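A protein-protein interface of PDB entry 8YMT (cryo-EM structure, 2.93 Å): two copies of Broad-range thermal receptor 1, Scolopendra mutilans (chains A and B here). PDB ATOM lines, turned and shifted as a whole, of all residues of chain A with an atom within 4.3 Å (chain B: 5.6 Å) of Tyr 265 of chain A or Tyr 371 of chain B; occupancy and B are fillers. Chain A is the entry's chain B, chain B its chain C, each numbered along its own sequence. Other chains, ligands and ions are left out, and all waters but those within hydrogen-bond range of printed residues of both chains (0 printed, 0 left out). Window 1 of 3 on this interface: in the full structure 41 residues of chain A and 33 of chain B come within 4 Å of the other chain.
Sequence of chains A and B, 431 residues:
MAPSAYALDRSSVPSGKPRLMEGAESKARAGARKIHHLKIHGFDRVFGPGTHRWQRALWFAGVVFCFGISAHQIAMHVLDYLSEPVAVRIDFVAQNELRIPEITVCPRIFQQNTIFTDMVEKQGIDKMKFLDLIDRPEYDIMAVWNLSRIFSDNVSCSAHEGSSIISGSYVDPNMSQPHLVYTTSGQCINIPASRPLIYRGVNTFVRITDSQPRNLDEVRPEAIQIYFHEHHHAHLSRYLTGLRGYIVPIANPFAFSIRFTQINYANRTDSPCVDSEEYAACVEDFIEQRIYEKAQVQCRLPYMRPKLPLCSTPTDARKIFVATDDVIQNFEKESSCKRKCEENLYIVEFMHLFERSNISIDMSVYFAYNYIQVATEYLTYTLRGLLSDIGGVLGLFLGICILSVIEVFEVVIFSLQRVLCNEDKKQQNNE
Ile 263 of chain A touches Phe 92 of chain B (CD1 to CB, 3.7 Å).
CD1 of Tyr 371 of chain B touches CD1 of Ile 263 of chain A (3.3 Å).
OH of Tyr 265 of chain A touches OH of Tyr 371 of chain B, 3.7 Å away.
Tyr 371 of chain B touches Leu 345 of chain A (CD2 to CD1, 3.4 Å).
OE2 of Glu 343 of chain A is in hydrogen-bond range of OH of Tyr 371 of chain B (2.5 Å).
Printed residues of chain B within 4 Å of Tyr 265 of chain A: Tyr 371 (3.7 Å).
Of chain A, only Ile 263, Tyr 265, Glu 343 and Leu 345 come within 4 Å of Tyr 371 of chain B.
Of the printed residues of chain A, Phe 92 of chain B touches Ile 263.
Of the printed residues of chain B, Ile 263 of chain A touches Phe 92 and Tyr 371.
Printed residues of chain B within 4 Å of Glu 343 of chain A: Tyr 371.
Printed residues of chain B within 4 Å of Leu 345 of chain A: Tyr 371 (3.4 Å).
The nearest printed residue of chain A that does not touch Tyr 371 of chain B is Lys 340 of chain A (6.8 Å).
The nearest printed residue of chain B that does not touch Glu 343 of chain A is Ala 94 of chain B (6.0 Å).
No position is printed for both chains.
Of the 5 pairs that touch across the chains among the printed residues, none has its exchanged pair printed and touching as well.
Printed residues of chain A that touch a printed residue of chain B: Ile 263, Tyr 265, Glu 343 and Leu 345.
Hydrophobic or aromatic side chains of chain A that line the printed part of chain B: Ile 263, Tyr 265 and Leu 345.
Hydrophobic or aromatic side chains of chain B within 4 Å of the printed part of chain A: Phe 92 and Tyr 371.
Among the printed residues, 5 pairs touch across the chains.
The backbone NH (N) of Tyr 265 of chain A is in hydrogen-bond range of the backbone carbonyl oxygen (O) of Cys 341 of chain A (2.7 Å).
The side-chain amino group of Lys 340 of chain A is in salt-bridge range of the side-chain carboxylate of Glu 343 of chain A.
The backbone carbonyl oxygen of Glu 343 of chain A is in hydrogen-bond range of the backbone NH of Ile 263 of chain A (2.9 Å).
SG of Cys 341 of chain A is disulfide-bonded to SG of Cys 273 of chain A, at 2.0 Å.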
ATOM      1  N   ILE A 263      -2.371  22.368  32.293  1.00  0.00           N
ATOM      2  CA  ILE A 263      -2.579  22.993  30.991  1.00  0.00           C
ATOM      3  C   ILE A 263      -3.164  24.381  31.204  1.00  0.00           C
ATOM      4  O   ILE A 263      -4.382  24.548  31.311  1.00  0.00           O
ATOM      5  CB  ILE A 263      -3.483  22.139  30.086  1.00  0.00           C
ATOM      6  CG1 ILE A 263      -2.758  20.850  29.696  1.00  0.00           C
ATOM      7  CG2 ILE A 263      -3.895  22.931  28.851  1.00  0.00           C
ATOM      8  CD1 ILE A 263      -3.614  19.868  28.939  1.00  0.00           C
ATOM      9  N   ASN A 264      -2.292  25.381  31.256  1.00  0.00           N
ATOM     10  CA  ASN A 264      -2.730  26.753  31.445  1.00  0.00           C
ATOM     11  C   ASN A 264      -3.159  27.357  30.115  1.00  0.00           C
ATOM     12  O   ASN A 264      -2.503  27.181  29.088  1.00  0.00           O
ATOM     13  CB  ASN A 264      -1.606  27.585  32.057  1.00  0.00           C
ATOM     14  CG  ASN A 264      -1.327  27.215  33.494  1.00  0.00           C
ATOM     15  OD1 ASN A 264      -2.240  27.113  34.311  1.00  0.00           O
ATOM     16  ND2 ASN A 264      -0.056  27.001  33.812  1.00  0.00           N
ATOM     17  N   TYR A 265      -4.271  28.084  30.142  1.00  0.00           N
ATOM     18  CA  TYR A 265      -4.800  28.746  28.961  1.00  0.00           C
ATOM     19  C   TYR A 265      -4.640  30.252  29.102  1.00  0.00           C
ATOM     20  O   TYR A 265      -4.500  30.785  30.206  1.00  0.00           O
ATOM     21  CB  TYR A 265      -6.274  28.392  28.737  1.00  0.00           C
ATOM     22  CG  TYR A 265      -6.493  26.963  28.301  1.00  0.00           C
ATOM     23  CD1 TYR A 265      -6.118  26.539  27.035  1.00  0.00           C
ATOM     24  CD2 TYR A 265      -7.071  26.036  29.157  1.00  0.00           C
ATOM     25  CE1 TYR A 265      -6.314  25.234  26.632  1.00  0.00           C
ATOM     26  CE2 TYR A 265      -7.270  24.728  28.763  1.00  0.00           C
ATOM     27  CZ  TYR A 265      -6.891  24.333  27.498  1.00  0.00           C
ATOM     28  OH  TYR A 265      -7.087  23.032  27.097  1.00  0.00           O
ATOM     29  N   ALA A 266      -4.661  30.936  27.962  1.00  0.00           N
ATOM     30  CA  ALA A 266      -4.480  32.380  27.907  1.00  0.00           C
ATOM     31  C   ALA A 266      -5.846  33.053  27.906  1.00  0.00           C
ATOM     32  O   ALA A 266      -6.683  32.766  27.044  1.00  0.00           O
ATOM     33  CB  ALA A 266      -3.681  32.783  26.669  1.00  0.00           C
ATOM     34  N   ASN A 267      -6.069  33.941  28.871  1.00  0.00           N
ATOM     35  CA  ASN A 267      -7.318  34.685  28.934  1.00  0.00           C
ATOM     36  C   ASN A 267      -7.348  35.715  27.812  1.00  0.00           C
ATOM     37  O   ASN A 267      -6.527  36.638  27.785  1.00  0.00           O
ATOM     38  CB  ASN A 267      -7.462  35.364  30.294  1.00  0.00           C
ATOM     39  CG  ASN A 267      -8.840  35.951  30.510  1.00  0.00           C
ATOM     40  OD1 ASN A 267      -9.624  36.086  29.571  1.00  0.00           O
ATOM     41  ND2 ASN A 267      -9.146  36.302  31.753  1.00  0.00           N
ATOM     42  N   CYS A 273     -10.728  32.339  29.617  1.00  0.00           N
ATOM     43  CA  CYS A 273     -10.623  31.396  30.717  1.00  0.00           C
ATOM     44  C   CYS A 273     -11.132  32.029  32.006  1.00  0.00           C
ATOM     45  O   CYS A 273     -10.985  33.231  32.235  1.00  0.00           O
ATOM     46  CB  CYS A 273      -9.175  30.939  30.891  1.00  0.00           C
ATOM     47  SG  CYS A 273      -8.103  32.141  31.719  1.00  0.00           S
ATOM     48  N   LYS A 340     -11.253  26.343  32.394  1.00  0.00           N
ATOM     49  CA  LYS A 340     -10.513  27.134  33.355  1.00  0.00           C
ATOM     50  C   LYS A 340      -9.253  27.696  32.710  1.00  0.00           C
ATOM     51  O   LYS A 340      -8.831  27.278  31.627  1.00  0.00           O
ATOM     52  CB  LYS A 340     -10.111  26.301  34.572  1.00  0.00           C
ATOM     53  CG  LYS A 340     -11.245  25.861  35.480  1.00  0.00           C
ATOM     54  CD  LYS A 340     -12.022  24.673  34.933  1.00  0.00           C
ATOM     55  CE  LYS A 340     -11.168  23.423  34.789  1.00  0.00           C
ATOM     56  NZ  LYS A 340     -11.974  22.263  34.329  1.00  0.00           N
ATOM     57  N   CYS A 341      -8.644  28.660  33.393  1.00  0.00           N
ATOM     58  CA  CYS A 341      -7.282  29.042  33.056  1.00  0.00           C
ATOM     59  C   CYS A 341      -6.327  27.897  33.363  1.00  0.00           C
ATOM     60  O   CYS A 341      -5.527  27.492  32.512  1.00  0.00           O
ATOM     61  CB  CYS A 341      -6.897  30.311  33.815  1.00  0.00           C
ATOM     62  SG  CYS A 341      -8.139  31.619  33.682  1.00  0.00           S
ATOM     63  N   GLU A 343      -5.848  23.935  34.046  1.00  0.00           N
ATOM     64  CA  GLU A 343      -6.501  22.661  33.733  1.00  0.00           C
ATOM     65  C   GLU A 343      -5.573  21.543  34.198  1.00  0.00           C
ATOM     66  O   GLU A 343      -4.736  21.062  33.430  1.00  0.00           O
ATOM     67  CB  GLU A 343      -6.810  22.564  32.237  1.00  0.00           C
ATOM     68  CG  GLU A 343      -7.263  21.192  31.749  1.00  0.00           C
ATOM     69  CD  GLU A 343      -8.756  20.985  31.884  1.00  0.00           C
ATOM     70  OE1 GLU A 343      -9.407  21.779  32.595  1.00  0.00           O
ATOM     71  OE2 GLU A 343      -9.282  20.031  31.275  1.00  0.00           O
ATOM     72  N   LEU A 345      -4.329  17.877  35.135  1.00  0.00           N
ATOM     73  CA  LEU A 345      -4.570  16.563  34.545  1.00  0.00           C
ATOM     74  C   LEU A 345      -3.763  15.539  35.329  1.00  0.00           C
ATOM     75  O   LEU A 345      -2.533  15.618  35.370  1.00  0.00           O
ATOM     76  CB  LEU A 345      -4.185  16.536  33.068  1.00  0.00           C
ATOM     77  CG  LEU A 345      -5.065  17.335  32.108  1.00  0.00           C
ATOM     78  CD1 LEU A 345      -4.476  17.274  30.713  1.00  0.00           C
ATOM     79  CD2 LEU A 345      -6.494  16.824  32.113  1.00  0.00           C
ATOM     80  N   GLU A 377      -0.562  28.285  27.273  1.00  0.00           N
ATOM     81  CA  GLU A 377      -0.926  29.098  26.126  1.00  0.00           C
ATOM     82  C   GLU A 377      -0.715  30.565  26.473  1.00  0.00           C
ATOM     83  O   GLU A 377      -1.052  31.006  27.576  1.00  0.00           O
ATOM     84  CB  GLU A 377      -2.384  28.849  25.743  1.00  0.00           C
ATOM     85  CG  GLU A 377      -2.679  28.997  24.273  1.00  0.00           C
ATOM     86  CD  GLU A 377      -4.086  28.561  23.915  1.00  0.00           C
ATOM     87  OE1 GLU A 377      -5.046  29.196  24.396  1.00  0.00           O
ATOM     88  OE2 GLU A 377      -4.230  27.584  23.153  1.00  0.00           O
ATOM     89  N   PHE B  92      -1.741  20.457  23.305  1.00  0.00           N
ATOM     90  CA  PHE B  92      -2.515  19.434  24.006  1.00  0.00           C
ATOM     91  C   PHE B  92      -3.976  19.604  23.597  1.00  0.00           C
ATOM     92  O   PHE B  92      -4.712  20.393  24.194  1.00  0.00           O
ATOM     93  CB  PHE B  92      -2.331  19.547  25.514  1.00  0.00           C
ATOM     94  CG  PHE B  92      -1.189  18.728  26.047  1.00  0.00           C
ATOM     95  CD1 PHE B  92       0.113  19.187  25.951  1.00  0.00           C
ATOM     96  CD2 PHE B  92      -1.418  17.501  26.643  1.00  0.00           C
ATOM     97  CE1 PHE B  92       1.166  18.438  26.440  1.00  0.00           C
ATOM     98  CE2 PHE B  92      -0.369  16.747  27.133  1.00  0.00           C
ATOM     99  CZ  PHE B  92       0.925  17.217  27.030  1.00  0.00           C
ATOM    100  N   VAL B  93      -4.389  18.856  22.578  1.00  0.00           N
ATOM    101  CA  VAL B  93      -5.729  18.977  22.004  1.00  0.00           C
ATOM    102  C   VAL B  93      -6.670  18.117  22.844  1.00  0.00           C
ATOM    103  O   VAL B  93      -6.492  16.904  22.950  1.00  0.00           O
ATOM    104  CB  VAL B  93      -5.755  18.561  20.532  1.00  0.00           C
ATOM    105  CG1 VAL B  93      -7.125  18.826  19.925  1.00  0.00           C
ATOM    106  CG2 VAL B  93      -4.670  19.285  19.753  1.00  0.00           C
ATOM    107  N   ALA B  94      -7.678  18.748  23.445  1.00  0.00           N
ATOM    108  CA  ALA B  94      -8.713  18.016  24.166  1.00  0.00           C
ATOM    109  C   ALA B  94      -9.876  17.714  23.234  1.00  0.00           C
ATOM    110  O   ALA B  94     -10.659  18.611  22.904  1.00  0.00           O
ATOM    111  CB  ALA B  94      -9.198  18.814  25.376  1.00  0.00           C
ATOM    112  N   GLN B  95      -9.999  16.464  22.803  1.00  0.00           N
ATOM    113  CA  GLN B  95     -11.038  16.059  21.871  1.00  0.00           C
ATOM    114  C   GLN B  95     -11.996  15.083  22.537  1.00  0.00           C
ATOM    115  O   GLN B  95     -11.579  14.106  23.165  1.00  0.00           O
ATOM    116  CB  GLN B  95     -10.435  15.417  20.620  1.00  0.00           C
ATOM    117  CG  GLN B  95      -9.684  14.124  20.886  1.00  0.00           C
ATOM    118  CD  GLN B  95      -8.516  13.917  19.941  1.00  0.00           C
ATOM    119  OE1 GLN B  95      -8.250  14.745  19.070  1.00  0.00           O
ATOM    120  NE2 GLN B  95      -7.811  12.805  20.109  1.00  0.00           N
ATOM    121  N   PHE B 260      -2.816   8.864  23.617  1.00  0.00           N
ATOM    122  CA  PHE B 260      -2.465   9.197  22.246  1.00  0.00           C
ATOM    123  C   PHE B 260      -1.400  10.284  22.213  1.00  0.00           C
ATOM    124  O   PHE B 260      -1.380  11.202  23.038  1.00  0.00           O
ATOM    125  CB  PHE B 260      -3.702   9.638  21.463  1.00  0.00           C
ATOM    126  CG  PHE B 260      -4.801   8.616  21.450  1.00  0.00           C
ATOM    127  CD1 PHE B 260      -5.850   8.694  22.348  1.00  0.00           C
ATOM    128  CD2 PHE B 260      -4.780   7.570  20.547  1.00  0.00           C
ATOM    129  CE1 PHE B 260      -6.857   7.753  22.338  1.00  0.00           C
ATOM    130  CE2 PHE B 260      -5.783   6.629  20.534  1.00  0.00           C
ATOM    131  CZ  PHE B 260      -6.823   6.721  21.430  1.00  0.00           C
ATOM    132  N   TYR B 369      -7.915   9.296  28.949  1.00  0.00           N
ATOM    133  CA  TYR B 369      -7.359  10.626  28.781  1.00  0.00           C
ATOM    134  C   TYR B 369      -7.641  11.101  27.364  1.00  0.00           C
ATOM    135  O   TYR B 369      -7.273  10.438  26.392  1.00  0.00           O
ATOM    136  CB  TYR B 369      -5.857  10.622  29.065  1.00  0.00           C
ATOM    137  CG  TYR B 369      -5.496   9.886  30.336  1.00  0.00           C
ATOM    138  CD1 TYR B 369      -5.967  10.315  31.569  1.00  0.00           C
ATOM    139  CD2 TYR B 369      -4.702   8.750  30.302  1.00  0.00           C
ATOM    140  CE1 TYR B 369      -5.642   9.642  32.731  1.00  0.00           C
ATOM    141  CE2 TYR B 369      -4.371   8.072  31.457  1.00  0.00           C
ATOM    142  CZ  TYR B 369      -4.844   8.521  32.669  1.00  0.00           C
ATOM    143  OH  TYR B 369      -4.517   7.844  33.820  1.00  0.00           O
ATOM    144  N   ASN B 370      -8.303  12.252  27.257  1.00  0.00           N
ATOM    145  CA  ASN B 370      -8.717  12.803  25.975  1.00  0.00           C
ATOM    146  C   ASN B 370      -7.780  13.883  25.456  1.00  0.00           C
ATOM    147  O   ASN B 370      -8.075  14.497  24.427  1.00  0.00           O
ATOM    148  CB  ASN B 370     -10.136  13.370  26.087  1.00  0.00           C
ATOM    149  CG  ASN B 370     -10.219  14.553  27.028  1.00  0.00           C
ATOM    150  OD1 ASN B 370      -9.508  14.613  28.031  1.00  0.00           O
ATOM    151  ND2 ASN B 370     -11.093  15.500  26.713  1.00  0.00           N
ATOM    152  N   TYR B 371      -6.657  14.126  26.135  1.00  0.00           N
ATOM    153  CA  TYR B 371      -5.719  15.173  25.737  1.00  0.00           C
ATOM    154  C   TYR B 371      -4.639  14.553  24.859  1.00  0.00           C
ATOM    155  O   TYR B 371      -3.567  14.150  25.314  1.00  0.00           O
ATOM    156  CB  TYR B 371      -5.129  15.850  26.965  1.00  0.00           C
ATOM    157  CG  TYR B 371      -5.980  16.972  27.504  1.00  0.00           C
ATOM    158  CD1 TYR B 371      -5.808  18.275  27.058  1.00  0.00           C
ATOM    159  CD2 TYR B 371      -6.969  16.728  28.443  1.00  0.00           C
ATOM    160  CE1 TYR B 371      -6.582  19.303  27.548  1.00  0.00           C
ATOM    161  CE2 TYR B 371      -7.751  17.750  28.933  1.00  0.00           C
ATOM    162  CZ  TYR B 371      -7.556  19.034  28.482  1.00  0.00           C
ATOM    163  OH  TYR B 371      -8.336  20.055  28.970  1.00  0.00           O
ATOM    164  N   ILE B 372      -4.936  14.477  23.563  1.00  0.00           N
ATOM    165  CA  ILE B 372      -3.970  13.990  22.586  1.00  0.00           C
ATOM    166  C   ILE B 372      -2.903  15.057  22.397  1.00  0.00           C
ATOM    167  O   ILE B 372      -3.174  16.135  21.859  1.00  0.00           O
ATOM    168  CB  ILE B 372      -4.647  13.627  21.250  1.00  0.00           C
ATOM    169  CG1 ILE B 372      -3.629  13.030  20.279  1.00  0.00           C
ATOM    170  CG2 ILE B 372      -5.309  14.841  20.615  1.00  0.00           C
ATOM    171  CD1 ILE B 372      -4.254  12.399  19.053  1.00  0.00           C
ATOM    172  N   GLN B 373      -1.687  14.782  22.861  1.00  0.00           N
ATOM    173  CA  GLN B 373      -0.602  15.730  22.669  1.00  0.00           C
ATOM    174  C   GLN B 373      -0.024  15.581  21.269  1.00  0.00           C
ATOM    175  O   GLN B 373       0.321  14.481  20.830  1.00  0.00           O
ATOM    176  CB  GLN B 373       0.488  15.533  23.722  1.00  0.00           C
ATOM    177  CG  GLN B 373       1.211  14.206  23.656  1.00  0.00           C
ATOM    178  CD  GLN B 373       2.235  14.054  24.765  1.00  0.00           C
ATOM    179  OE1 GLN B 373       2.452  14.974  25.552  1.00  0.00           O
ATOM    180  NE2 GLN B 373       2.865  12.888  24.833  1.00  0.00           N
